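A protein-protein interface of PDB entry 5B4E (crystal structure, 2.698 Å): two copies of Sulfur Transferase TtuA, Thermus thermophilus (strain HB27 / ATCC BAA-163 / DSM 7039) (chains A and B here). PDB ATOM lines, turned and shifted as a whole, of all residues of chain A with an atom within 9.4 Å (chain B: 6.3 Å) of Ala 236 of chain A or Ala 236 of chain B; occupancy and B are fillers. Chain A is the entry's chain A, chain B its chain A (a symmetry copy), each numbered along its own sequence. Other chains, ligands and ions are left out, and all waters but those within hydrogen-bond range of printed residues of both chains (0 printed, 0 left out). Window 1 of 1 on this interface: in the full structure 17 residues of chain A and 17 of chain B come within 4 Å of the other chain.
Of the 25 printed residues of chain A, 8 touch a printed residue of chain B. Along chain B the printed residues that touch a printed residue of chain A span positions 167 to 240. Among the printed residues, 12 pairs touch across the chains. Among the printed residues, no Asp or Glu carboxylate lies within 4 Å of a Lys or Arg side-chain nitrogen of the other chain.
Printed residues of chain B within 4 Å of Leu 171 of chain A: Val 240. Of the printed residues of chain B, Glu 235 of chain A touches Leu 239. Of the printed residues of chain B, Ala 236 of chain A touches Ala 236 and Leu 239. Of the printed residues of chain B, Val 240 of chain A touches Leu 232 (3.7 Å). Ala 236 of chain B touches just these residues of chain A: Ala 236 (3.6 Å) and Leu 239 (3.9 Å).
Among the printed residues, pairs that only touch across the chains: Leu 171 of chain A with Val 240 of chain B (3.6 Å), Ala 236 of chain A with Ala 236 of chain B (3.6 Å), Leu 232 of chain A with Leu 239 of chain B (3.6 Å), Leu 239 of chain A with Leu 232 of chain B (3.6 Å), Leu 232 of chain A with Val 240 of chain B (3.7 Å), Val 240 of chain A with Leu 232 of chain B (3.7 Å), Glu 235 of chain A with Leu 239 of chain B (3.7 Å), Leu 239 of chain A with Glu 235 of chain B (3.7 Å), Phe 167 of chain A with Phe 167 of chain B (3.9 Å), Ser 243 of chain A with Leu 232 of chain B (3.9 Å), Ala 236 of chain A with Leu 239 of chain B (3.9 Å) and Leu 239 of chain A with Ala 236 of chain B (3.9 Å).
Phe 167 of chain B touches its own counterpart, Phe 167 of chain A. Leu 232 of chain A touches Leu 239 of chain B, and with the chains exchanged Leu 239 of chain A touches Leu 232 of chain B. Glu 235 of chain A touches Leu 239 of chain B, and with the chains exchanged Leu 239 of chain A touches Glu 235 of chain B. Ala 236 of chain A touches Leu 239 of chain B, and with the chains exchanged Leu 239 of chain A touches Ala 236 of chain B. Positions printed for both chains: 167, 231, 232, 233, 234, 235, 236, 237, 238, 239, 240 and 241. Of the 12 pairs that touch across the chains among the printed residues, 10 have their exchanged pair printed and touching as well.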
ATOM      1  N   ASP A 160      24.835  17.021  24.130  1.00  0.00           N
ATOM      2  CA  ASP A 160      24.252  16.686  22.836  1.00  0.00           C
ATOM      3  C   ASP A 160      22.882  16.043  23.022  1.00  0.00           C
ATOM      4  O   ASP A 160      21.935  16.359  22.304  1.00  0.00           O
ATOM      5  CB  ASP A 160      25.169  15.749  22.045  1.00  0.00           C
ATOM      6  CG  ASP A 160      26.386  16.457  21.484  1.00  0.00           C
ATOM      7  OD1 ASP A 160      26.929  17.343  22.174  1.00  0.00           O
ATOM      8  OD2 ASP A 160      26.796  16.129  20.350  1.00  0.00           O
ATOM      9  N   ALA A 163      20.338  18.775  24.421  1.00  0.00           N
ATOM     10  CA  ALA A 163      19.996  19.763  23.407  1.00  0.00           C
ATOM     11  C   ALA A 163      19.166  19.136  22.291  1.00  0.00           C
ATOM     12  O   ALA A 163      18.327  19.800  21.685  1.00  0.00           O
ATOM     13  CB  ALA A 163      21.254  20.406  22.842  1.00  0.00           C
ATOM     14  N   ALA A 164      19.401  17.856  22.018  1.00  0.00           N
ATOM     15  CA  ALA A 164      18.616  17.144  21.015  1.00  0.00           C
ATOM     16  C   ALA A 164      17.175  16.965  21.486  1.00  0.00           C
ATOM     17  O   ALA A 164      16.237  17.105  20.701  1.00  0.00           O
ATOM     18  CB  ALA A 164      19.243  15.796  20.699  1.00  0.00           C
ATOM     19  N   PHE A 167      15.497  20.385  21.347  1.00  0.00           N
ATOM     20  CA  PHE A 167      15.246  20.691  19.944  1.00  0.00           C
ATOM     21  C   PHE A 167      14.029  19.923  19.435  1.00  0.00           C
ATOM     22  O   PHE A 167      13.149  20.491  18.783  1.00  0.00           O
ATOM     23  CB  PHE A 167      16.478  20.350  19.102  1.00  0.00           C
ATOM     24  CG  PHE A 167      16.446  20.917  17.711  1.00  0.00           C
ATOM     25  CD1 PHE A 167      15.690  22.039  17.420  1.00  0.00           C
ATOM     26  CD2 PHE A 167      17.172  20.321  16.693  1.00  0.00           C
ATOM     27  CE1 PHE A 167      15.663  22.560  16.140  1.00  0.00           C
ATOM     28  CE2 PHE A 167      17.148  20.836  15.411  1.00  0.00           C
ATOM     29  CZ  PHE A 167      16.394  21.957  15.134  1.00  0.00           C
ATOM     30  N   GLY A 168      13.988  18.631  19.748  1.00  0.00           N
ATOM     31  CA  GLY A 168      12.909  17.760  19.315  1.00  0.00           C
ATOM     32  C   GLY A 168      11.548  18.175  19.835  1.00  0.00           C
ATOM     33  O   GLY A 168      10.560  18.123  19.107  1.00  0.00           O
ATOM     34  N   LEU A 171      10.353  21.206  17.788  1.00  0.00           N
ATOM     35  CA  LEU A 171       9.920  20.847  16.444  1.00  0.00           C
ATOM     36  C   LEU A 171       8.753  19.869  16.476  1.00  0.00           C
ATOM     37  O   LEU A 171       7.928  19.843  15.563  1.00  0.00           O
ATOM     38  CB  LEU A 171      11.074  20.236  15.651  1.00  0.00           C
ATOM     39  CG  LEU A 171      12.377  21.028  15.568  1.00  0.00           C
ATOM     40  CD1 LEU A 171      13.392  20.258  14.750  1.00  0.00           C
ATOM     41  CD2 LEU A 171      12.143  22.398  14.965  1.00  0.00           C
ATOM     42  N   ALA A 228      16.902   7.102  15.835  1.00  0.00           N
ATOM     43  CA  ALA A 228      17.313   7.697  14.574  1.00  0.00           C
ATOM     44  C   ALA A 228      16.857   9.145  14.548  1.00  0.00           C
ATOM     45  O   ALA A 228      17.385   9.963  13.802  1.00  0.00           O
ATOM     46  CB  ALA A 228      16.728   6.932  13.408  1.00  0.00           C
ATOM     47  N   LYS A 229      15.841   9.453  15.340  1.00  0.00           N
ATOM     48  CA  LYS A 229      15.409  10.819  15.532  1.00  0.00           C
ATOM     49  C   LYS A 229      16.400  11.707  16.265  1.00  0.00           C
ATOM     50  O   LYS A 229      16.755  12.767  15.798  1.00  0.00           O
ATOM     51  CB  LYS A 229      14.129  10.802  16.332  1.00  0.00           C
ATOM     52  CG  LYS A 229      12.878  10.837  15.503  1.00  0.00           C
ATOM     53  CD  LYS A 229      11.772  11.511  16.274  1.00  0.00           C
ATOM     54  CE  LYS A 229      11.010  10.532  17.133  1.00  0.00           C
ATOM     55  NZ  LYS A 229       9.621  10.350  16.633  1.00  0.00           N
ATOM     56  N   SER A 230      16.907  11.227  17.386  1.00  0.00           N
ATOM     57  CA  SER A 230      17.905  11.969  18.146  1.00  0.00           C
ATOM     58  C   SER A 230      19.159  12.221  17.310  1.00  0.00           C
ATOM     59  O   SER A 230      19.771  13.284  17.400  1.00  0.00           O
ATOM     60  CB  SER A 230      18.263  11.213  19.425  1.00  0.00           C
ATOM     61  OG  SER A 230      19.030  10.055  19.140  1.00  0.00           O
ATOM     62  N   LEU A 231      19.526  11.237  16.494  1.00  0.00           N
ATOM     63  CA  LEU A 231      20.673  11.359  15.599  1.00  0.00           C
ATOM     64  C   LEU A 231      20.430  12.469  14.577  1.00  0.00           C
ATOM     65  O   LEU A 231      21.366  13.180  14.192  1.00  0.00           O
ATOM     66  CB  LEU A 231      20.959  10.030  14.887  1.00  0.00           C
ATOM     67  CG  LEU A 231      21.280   8.831  15.788  1.00  0.00           C
ATOM     68  CD1 LEU A 231      21.443   7.529  15.002  1.00  0.00           C
ATOM     69  CD2 LEU A 231      22.512   9.096  16.639  1.00  0.00           C
ATOM     70  N   LEU A 232      19.177  12.619  14.145  1.00  0.00           N
ATOM     71  CA  LEU A 232      18.813  13.695  13.229  1.00  0.00           C
ATOM     72  C   LEU A 232      18.927  15.057  13.910  1.00  0.00           C
ATOM     73  O   LEU A 232      19.456  16.008  13.335  1.00  0.00           O
ATOM     74  CB  LEU A 232      17.395  13.485  12.700  1.00  0.00           C
ATOM     75  CG  LEU A 232      16.895  14.488  11.661  1.00  0.00           C
ATOM     76  CD1 LEU A 232      17.667  14.335  10.356  1.00  0.00           C
ATOM     77  CD2 LEU A 232      15.397  14.350  11.423  1.00  0.00           C
ATOM     78  N   TYR A 233      18.421  15.143  15.136  1.00  0.00           N
ATOM     79  CA  TYR A 233      18.521  16.362  15.931  1.00  0.00           C
ATOM     80  C   TYR A 233      19.976  16.743  16.197  1.00  0.00           C
ATOM     81  O   TYR A 233      20.336  17.917  16.158  1.00  0.00           O
ATOM     82  CB  TYR A 233      17.782  16.194  17.259  1.00  0.00           C
ATOM     83  CG  TYR A 233      16.309  15.900  17.118  1.00  0.00           C
ATOM     84  CD1 TYR A 233      15.582  16.393  16.041  1.00  0.00           C
ATOM     85  CD2 TYR A 233      15.643  15.134  18.062  1.00  0.00           C
ATOM     86  CE1 TYR A 233      14.232  16.129  15.910  1.00  0.00           C
ATOM     87  CE2 TYR A 233      14.296  14.863  17.940  1.00  0.00           C
ATOM     88  CZ  TYR A 233      13.595  15.363  16.862  1.00  0.00           C
ATOM     89  OH  TYR A 233      12.252  15.097  16.737  1.00  0.00           O
ATOM     90  N   LYS A 234      20.809  15.742  16.469  1.00  0.00           N
ATOM     91  CA  LYS A 234      22.216  15.981  16.764  1.00  0.00           C
ATOM     92  C   LYS A 234      22.959  16.482  15.533  1.00  0.00           C
ATOM     93  O   LYS A 234      23.801  17.374  15.631  1.00  0.00           O
ATOM     94  CB  LYS A 234      22.880  14.712  17.300  1.00  0.00           C
ATOM     95  CG  LYS A 234      22.430  14.318  18.694  1.00  0.00           C
ATOM     96  CD  LYS A 234      23.138  13.064  19.171  1.00  0.00           C
ATOM     97  CE  LYS A 234      22.718  12.709  20.584  1.00  0.00           C
ATOM     98  NZ  LYS A 234      23.582  11.653  21.179  1.00  0.00           N
ATOM     99  N   GLU A 235      22.647  15.903  14.379  1.00  0.00           N
ATOM    100  CA  GLU A 235      23.243  16.339  13.122  1.00  0.00           C
ATOM    101  C   GLU A 235      22.942  17.808  12.857  1.00  0.00           C
ATOM    102  O   GLU A 235      23.826  18.574  12.474  1.00  0.00           O
ATOM    103  CB  GLU A 235      22.736  15.487  11.958  1.00  0.00           C
ATOM    104  CG  GLU A 235      23.345  14.100  11.874  1.00  0.00           C
ATOM    105  CD  GLU A 235      22.755  13.284  10.742  1.00  0.00           C
ATOM    106  OE1 GLU A 235      21.739  13.721  10.162  1.00  0.00           O
ATOM    107  OE2 GLU A 235      23.308  12.209  10.427  1.00  0.00           O
ATOM    108  N   ALA A 236      21.688  18.190  13.069  1.00  0.00           N
ATOM    109  CA  ALA A 236      21.252  19.565  12.857  1.00  0.00           C
ATOM    110  C   ALA A 236      21.974  20.525  13.802  1.00  0.00           C
ATOM    111  O   ALA A 236      22.495  21.554  13.373  1.00  0.00           O
ATOM    112  CB  ALA A 236      19.742  19.675  13.035  1.00  0.00           C
ATOM    113  N   LEU A 237      22.002  20.181  15.085  1.00  0.00           N
ATOM    114  CA  LEU A 237      22.640  21.027  16.086  1.00  0.00           C
ATOM    115  C   LEU A 237      24.155  21.105  15.887  1.00  0.00           C
ATOM    116  O   LEU A 237      24.744  22.179  15.992  1.00  0.00           O
ATOM    117  CB  LEU A 237      22.317  20.518  17.493  1.00  0.00           C
ATOM    118  CG  LEU A 237      20.853  20.635  17.928  1.00  0.00           C
ATOM    119  CD1 LEU A 237      20.613  19.873  19.219  1.00  0.00           C
ATOM    120  CD2 LEU A 237      20.447  22.093  18.085  1.00  0.00           C
ATOM    121  N   ASN A 238      24.782  19.971  15.589  1.00  0.00           N
ATOM    122  CA  ASN A 238      26.232  19.941  15.406  1.00  0.00           C
ATOM    123  C   ASN A 238      26.681  20.664  14.142  1.00  0.00           C
ATOM    124  O   ASN A 238      27.802  21.171  14.076  1.00  0.00           O
ATOM    125  CB  ASN A 238      26.740  18.498  15.391  1.00  0.00           C
ATOM    126  CG  ASN A 238      26.813  17.898  16.781  1.00  0.00           C
ATOM    127  OD1 ASN A 238      27.097  18.597  17.755  1.00  0.00           O
ATOM    128  ND2 ASN A 238      26.553  16.599  16.883  1.00  0.00           N
ATOM    129  N   LEU A 239      25.805  20.708  13.141  1.00  0.00           N
ATOM    130  CA  LEU A 239      26.082  21.457  11.921  1.00  0.00           C
ATOM    131  C   LEU A 239      26.295  22.928  12.251  1.00  0.00           C
ATOM    132  O   LEU A 239      27.204  23.573  11.726  1.00  0.00           O
ATOM    133  CB  LEU A 239      24.939  21.303  10.917  1.00  0.00           C
ATOM    134  CG  LEU A 239      25.109  22.060   9.598  1.00  0.00           C
ATOM    135  CD1 LEU A 239      26.174  21.406   8.728  1.00  0.00           C
ATOM    136  CD2 LEU A 239      23.786  22.160   8.856  1.00  0.00           C
ATOM    137  N   VAL A 240      25.450  23.450  13.131  1.00  0.00           N
ATOM    138  CA  VAL A 240      25.570  24.827  13.581  1.00  0.00           C
ATOM    139  C   VAL A 240      26.779  24.980  14.495  1.00  0.00           C
ATOM    140  O   VAL A 240      27.563  25.919  14.349  1.00  0.00           O
ATOM    141  CB  VAL A 240      24.303  25.292  14.323  1.00  0.00           C
ATOM    142  CG1 VAL A 240      24.530  26.652  14.957  1.00  0.00           C
ATOM    143  CG2 VAL A 240      23.119  25.334  13.370  1.00  0.00           C
ATOM    144  N   GLU A 241      26.924  24.041  15.428  1.00  0.00           N
ATOM    145  CA  GLU A 241      28.030  24.037  16.384  1.00  0.00           C
ATOM    146  C   GLU A 241      29.386  24.104  15.686  1.00  0.00           C
ATOM    147  O   GLU A 241      30.304  24.778  16.155  1.00  0.00           O
ATOM    148  CB  GLU A 241      27.954  22.786  17.267  1.00  0.00           C
ATOM    149  CG  GLU A 241      29.026  22.701  18.341  1.00  0.00           C
ATOM    150  CD  GLU A 241      28.787  23.667  19.483  1.00  0.00           C
ATOM    151  OE1 GLU A 241      29.739  23.935  20.249  1.00  0.00           O
ATOM    152  OE2 GLU A 241      27.644  24.156  19.620  1.00  0.00           O
ATOM    153  N   ARG A 242      29.495  23.409  14.560  1.00  0.00           N
ATOM    154  CA  ARG A 242      30.731  23.355  13.789  1.00  0.00           C
ATOM    155  C   ARG A 242      31.208  24.745  13.365  1.00  0.00           C
ATOM    156  O   ARG A 242      32.395  25.061  13.464  1.00  0.00           O
ATOM    157  CB  ARG A 242      30.534  22.469  12.557  1.00  0.00           C
ATOM    158  CG  ARG A 242      31.818  21.980  11.921  1.00  0.00           C
ATOM    159  CD  ARG A 242      31.527  20.916  10.874  1.00  0.00           C
ATOM    160  NE  ARG A 242      30.897  21.474   9.680  1.00  0.00           N
ATOM    161  CZ  ARG A 242      30.352  20.742   8.713  1.00  0.00           C
ATOM    162  NH1 ARG A 242      30.349  19.419   8.805  1.00  0.00           N
ATOM    163  NH2 ARG A 242      29.804  21.332   7.662  1.00  0.00           N
ATOM    164  N   SER A 243      30.274  25.573  12.906  1.00  0.00           N
ATOM    165  CA  SER A 243      30.596  26.916  12.434  1.00  0.00           C
ATOM    166  C   SER A 243      30.466  27.963  13.534  1.00  0.00           C
ATOM    167  O   SER A 243      30.977  29.075  13.404  1.00  0.00           O
ATOM    168  CB  SER A 243      29.692  27.300  11.260  1.00  0.00           C
ATOM    169  OG  SER A 243      29.796  26.368  10.197  1.00  0.00           O
ATOM    170  N   ALA A 247      27.154  26.895  20.609  1.00  0.00           N
ATOM    171  CA  ALA A 247      25.748  26.967  20.217  1.00  0.00           C
ATOM    172  C   ALA A 247      24.866  26.071  21.084  1.00  0.00           C
ATOM    173  O   ALA A 247      23.851  26.519  21.612  1.00  0.00           O
ATOM    174  CB  ALA A 247      25.591  26.599  18.752  1.00  0.00           C
ATOM    175  N   LYS A 248      25.256  24.807  21.226  1.00  0.00           N
ATOM    176  CA  LYS A 248      24.502  23.870  22.055  1.00  0.00           C
ATOM    177  C   LYS A 248      24.446  24.339  23.504  1.00  0.00           C
ATOM    178  O   LYS A 248      23.393  24.279  24.139  1.00  0.00           O
ATOM    179  CB  LYS A 248      25.110  22.469  21.981  1.00  0.00           C
ATOM    180  CG  LYS A 248      25.005  21.826  20.613  1.00  0.00           C
ATOM    181  CD  LYS A 248      25.657  20.456  20.592  1.00  0.00           C
ATOM    182  CE  LYS A 248      27.140  20.544  20.909  1.00  0.00           C
ATOM    183  NZ  LYS A 248      27.834  19.259  20.632  1.00  0.00           N
ATOM    184  N   PHE A 251      22.167  27.307  23.637  1.00  0.00           N
ATOM    185  CA  PHE A 251      20.822  26.774  23.454  1.00  0.00           C
ATOM    186  C   PHE A 251      20.276  26.182  24.749  1.00  0.00           C
ATOM    187  O   PHE A 251      19.226  26.594  25.242  1.00  0.00           O
ATOM    188  CB  PHE A 251      20.832  25.716  22.347  1.00  0.00           C
ATOM    189  CG  PHE A 251      19.471  25.206  21.969  1.00  0.00           C
ATOM    190  CD1 PHE A 251      18.449  26.083  21.655  1.00  0.00           C
ATOM    191  CD2 PHE A 251      19.226  23.843  21.894  1.00  0.00           C
ATOM    192  CE1 PHE A 251      17.199  25.611  21.296  1.00  0.00           C
ATOM    193  CE2 PHE A 251      17.981  23.366  21.533  1.00  0.00           C
ATOM    194  CZ  PHE A 251      16.966  24.251  21.235  1.00  0.00           C
ATOM    195  N   PHE B 167      15.315  30.141  15.248  1.00  0.00           N
ATOM    196  CA  PHE B 167      16.360  29.180  15.580  1.00  0.00           C
ATOM    197  C   PHE B 167      17.636  29.900  16.010  1.00  0.00           C
ATOM    198  O   PHE B 167      18.247  29.553  17.024  1.00  0.00           O
ATOM    199  CB  PHE B 167      16.643  28.273  14.380  1.00  0.00           C
ATOM    200  CG  PHE B 167      17.461  27.058  14.710  1.00  0.00           C
ATOM    201  CD1 PHE B 167      17.481  26.542  15.995  1.00  0.00           C
ATOM    202  CD2 PHE B 167      18.216  26.431  13.731  1.00  0.00           C
ATOM    203  CE1 PHE B 167      18.233  25.423  16.296  1.00  0.00           C
ATOM    204  CE2 PHE B 167      18.972  25.314  14.026  1.00  0.00           C
ATOM    205  CZ  PHE B 167      18.981  24.808  15.309  1.00  0.00           C
ATOM    206  N   LEU B 231      21.643  30.749   6.134  1.00  0.00           N
ATOM    207  CA  LEU B 231      21.786  29.565   5.292  1.00  0.00           C
ATOM    208  C   LEU B 231      22.154  28.351   6.145  1.00  0.00           C
ATOM    209  O   LEU B 231      21.715  27.231   5.859  1.00  0.00           O
ATOM    210  CB  LEU B 231      22.839  29.791   4.198  1.00  0.00           C
ATOM    211  CG  LEU B 231      22.571  30.946   3.225  1.00  0.00           C
ATOM    212  CD1 LEU B 231      23.721  31.164   2.241  1.00  0.00           C
ATOM    213  CD2 LEU B 231      21.262  30.743   2.477  1.00  0.00           C
ATOM    214  N   LEU B 232      22.953  28.576   7.189  1.00  0.00           N
ATOM    215  CA  LEU B 232      23.308  27.508   8.118  1.00  0.00           C
ATOM    216  C   LEU B 232      22.092  27.055   8.922  1.00  0.00           C
ATOM    217  O   LEU B 232      21.860  25.858   9.096  1.00  0.00           O
ATOM    218  CB  LEU B 232      24.422  27.969   9.056  1.00  0.00           C
ATOM    219  CG  LEU B 232      24.964  26.931  10.038  1.00  0.00           C
ATOM    220  CD1 LEU B 232      25.712  25.831   9.294  1.00  0.00           C
ATOM    221  CD2 LEU B 232      25.854  27.570  11.096  1.00  0.00           C
ATOM    222  N   TYR B 233      21.322  28.019   9.416  1.00  0.00           N
ATOM    223  CA  TYR B 233      20.092  27.733  10.145  1.00  0.00           C
ATOM    224  C   TYR B 233      19.085  26.982   9.275  1.00  0.00           C
ATOM    225  O   TYR B 233      18.407  26.071   9.743  1.00  0.00           O
ATOM    226  CB  TYR B 233      19.464  29.029  10.660  1.00  0.00           C
ATOM    227  CG  TYR B 233      20.342  29.812  11.604  1.00  0.00           C
ATOM    228  CD1 TYR B 233      21.252  29.168  12.434  1.00  0.00           C
ATOM    229  CD2 TYR B 233      20.260  31.194  11.667  1.00  0.00           C
ATOM    230  CE1 TYR B 233      22.055  29.883  13.303  1.00  0.00           C
ATOM    231  CE2 TYR B 233      21.059  31.917  12.529  1.00  0.00           C
ATOM    232  CZ  TYR B 233      21.955  31.257  13.345  1.00  0.00           C
ATOM    233  OH  TYR B 233      22.752  31.973  14.206  1.00  0.00           O
ATOM    234  N   LYS B 234      18.990  27.375   8.008  1.00  0.00           N
ATOM    235  CA  LYS B 234      18.047  26.753   7.086  1.00  0.00           C
ATOM    236  C   LYS B 234      18.443  25.314   6.783  1.00  0.00           C
ATOM    237  O   LYS B 234      17.586  24.434   6.705  1.00  0.00           O
ATOM    238  CB  LYS B 234      17.948  27.557   5.789  1.00  0.00           C
ATOM    239  CG  LYS B 234      17.251  28.895   5.941  1.00  0.00           C
ATOM    240  CD  LYS B 234      17.172  29.632   4.617  1.00  0.00           C
ATOM    241  CE  LYS B 234      16.430  30.945   4.771  1.00  0.00           C
ATOM    242  NZ  LYS B 234      16.099  31.562   3.457  1.00  0.00           N
ATOM    243  N   GLU B 235      19.739  25.082   6.610  1.00  0.00           N
ATOM    244  CA  GLU B 235      20.247  23.736   6.378  1.00  0.00           C
ATOM    245  C   GLU B 235      19.888  22.810   7.533  1.00  0.00           C
ATOM    246  O   GLU B 235      19.444  21.682   7.323  1.00  0.00           O
ATOM    247  CB  GLU B 235      21.763  23.755   6.181  1.00  0.00           C
ATOM    248  CG  GLU B 235      22.221  24.263   4.827  1.00  0.00           C
ATOM    249  CD  GLU B 235      23.731  24.320   4.718  1.00  0.00           C
ATOM    250  OE1 GLU B 235      24.407  24.163   5.757  1.00  0.00           O
ATOM    251  OE2 GLU B 235      24.243  24.517   3.596  1.00  0.00           O
ATOM    252  N   ALA B 236      20.081  23.302   8.752  1.00  0.00           N
ATOM    253  CA  ALA B 236      19.783  22.534   9.953  1.00  0.00           C
ATOM    254  C   ALA B 236      18.293  22.206  10.045  1.00  0.00           C
ATOM    255  O   ALA B 236      17.915  21.060  10.279  1.00  0.00           O
ATOM    256  CB  ALA B 236      20.240  23.291  11.195  1.00  0.00           C
ATOM    257  N   LEU B 237      17.454  23.218   9.855  1.00  0.00           N
ATOM    258  CA  LEU B 237      16.010  23.038   9.940  1.00  0.00           C
ATOM    259  C   LEU B 237      15.478  22.149   8.814  1.00  0.00           C
ATOM    260  O   LEU B 237      14.638  21.281   9.046  1.00  0.00           O
ATOM    261  CB  LEU B 237      15.304  24.395   9.921  1.00  0.00           C
ATOM    262  CG  LEU B 237      15.540  25.290  11.141  1.00  0.00           C
ATOM    263  CD1 LEU B 237      15.007  26.689  10.893  1.00  0.00           C
ATOM    264  CD2 LEU B 237      14.905  24.690  12.388  1.00  0.00           C
ATOM    265  N   ASN B 238      15.973  22.357   7.598  1.00  0.00           N
ATOM    266  CA  ASN B 238      15.508  21.577   6.454  1.00  0.00           C
ATOM    267  C   ASN B 238      15.950  20.119   6.517  1.00  0.00           C
ATOM    268  O   ASN B 238      15.282  19.238   5.972  1.00  0.00           O
ATOM    269  CB  ASN B 238      15.982  22.209   5.144  1.00  0.00           C
ATOM    270  CG  ASN B 238      15.162  23.425   4.762  1.00  0.00           C
ATOM    271  OD1 ASN B 238      13.960  23.483   5.025  1.00  0.00           O
ATOM    272  ND2 ASN B 238      15.807  24.406   4.140  1.00  0.00           N
ATOM    273  N   LEU B 239      17.075  19.869   7.180  1.00  0.00           N
ATOM    274  CA  LEU B 239      17.544  18.505   7.395  1.00  0.00           C
ATOM    275  C   LEU B 239      16.505  17.714   8.179  1.00  0.00           C
ATOM    276  O   LEU B 239      16.218  16.558   7.867  1.00  0.00           O
ATOM    277  CB  LEU B 239      18.880  18.499   8.138  1.00  0.00           C
ATOM    278  CG  LEU B 239      19.468  17.118   8.436  1.00  0.00           C
ATOM    279  CD1 LEU B 239      19.991  16.463   7.165  1.00  0.00           C
ATOM    280  CD2 LEU B 239      20.559  17.209   9.491  1.00  0.00           C
ATOM    281  N   VAL B 240      15.942  18.353   9.198  1.00  0.00           N
ATOM    282  CA  VAL B 240      14.895  17.740   9.997  1.00  0.00           C
ATOM    283  C   VAL B 240      13.601  17.658   9.198  1.00  0.00           C
ATOM    284  O   VAL B 240      12.935  16.622   9.185  1.00  0.00           O
ATOM    285  CB  VAL B 240      14.647  18.526  11.299  1.00  0.00           C
ATOM    286  CG1 VAL B 240      13.420  17.989  12.013  1.00  0.00           C
ATOM    287  CG2 VAL B 240      15.869  18.452  12.201  1.00  0.00           C
ATOM    288  N   GLU B 241      13.262  18.756   8.527  1.00  0.00           N
ATOM    289  CA  GLU B 241      12.053  18.845   7.710  1.00  0.00           C
ATOM    290  C   GLU B 241      11.979  17.722   6.679  1.00  0.00           C
ATOM    291  O   GLU B 241      10.907  17.176   6.418  1.00  0.00           O
ATOM    292  CB  GLU B 241      11.995  20.207   7.009  1.00  0.00           C
ATOM    293  CG  GLU B 241      10.748  20.436   6.170  1.00  0.00           C
ATOM    294  CD  GLU B 241       9.514  20.685   7.013  1.00  0.00           C
ATOM    295  OE1 GLU B 241       8.390  20.559   6.480  1.00  0.00           O
ATOM    296  OE2 GLU B 241       9.667  21.012   8.211  1.00  0.00           O
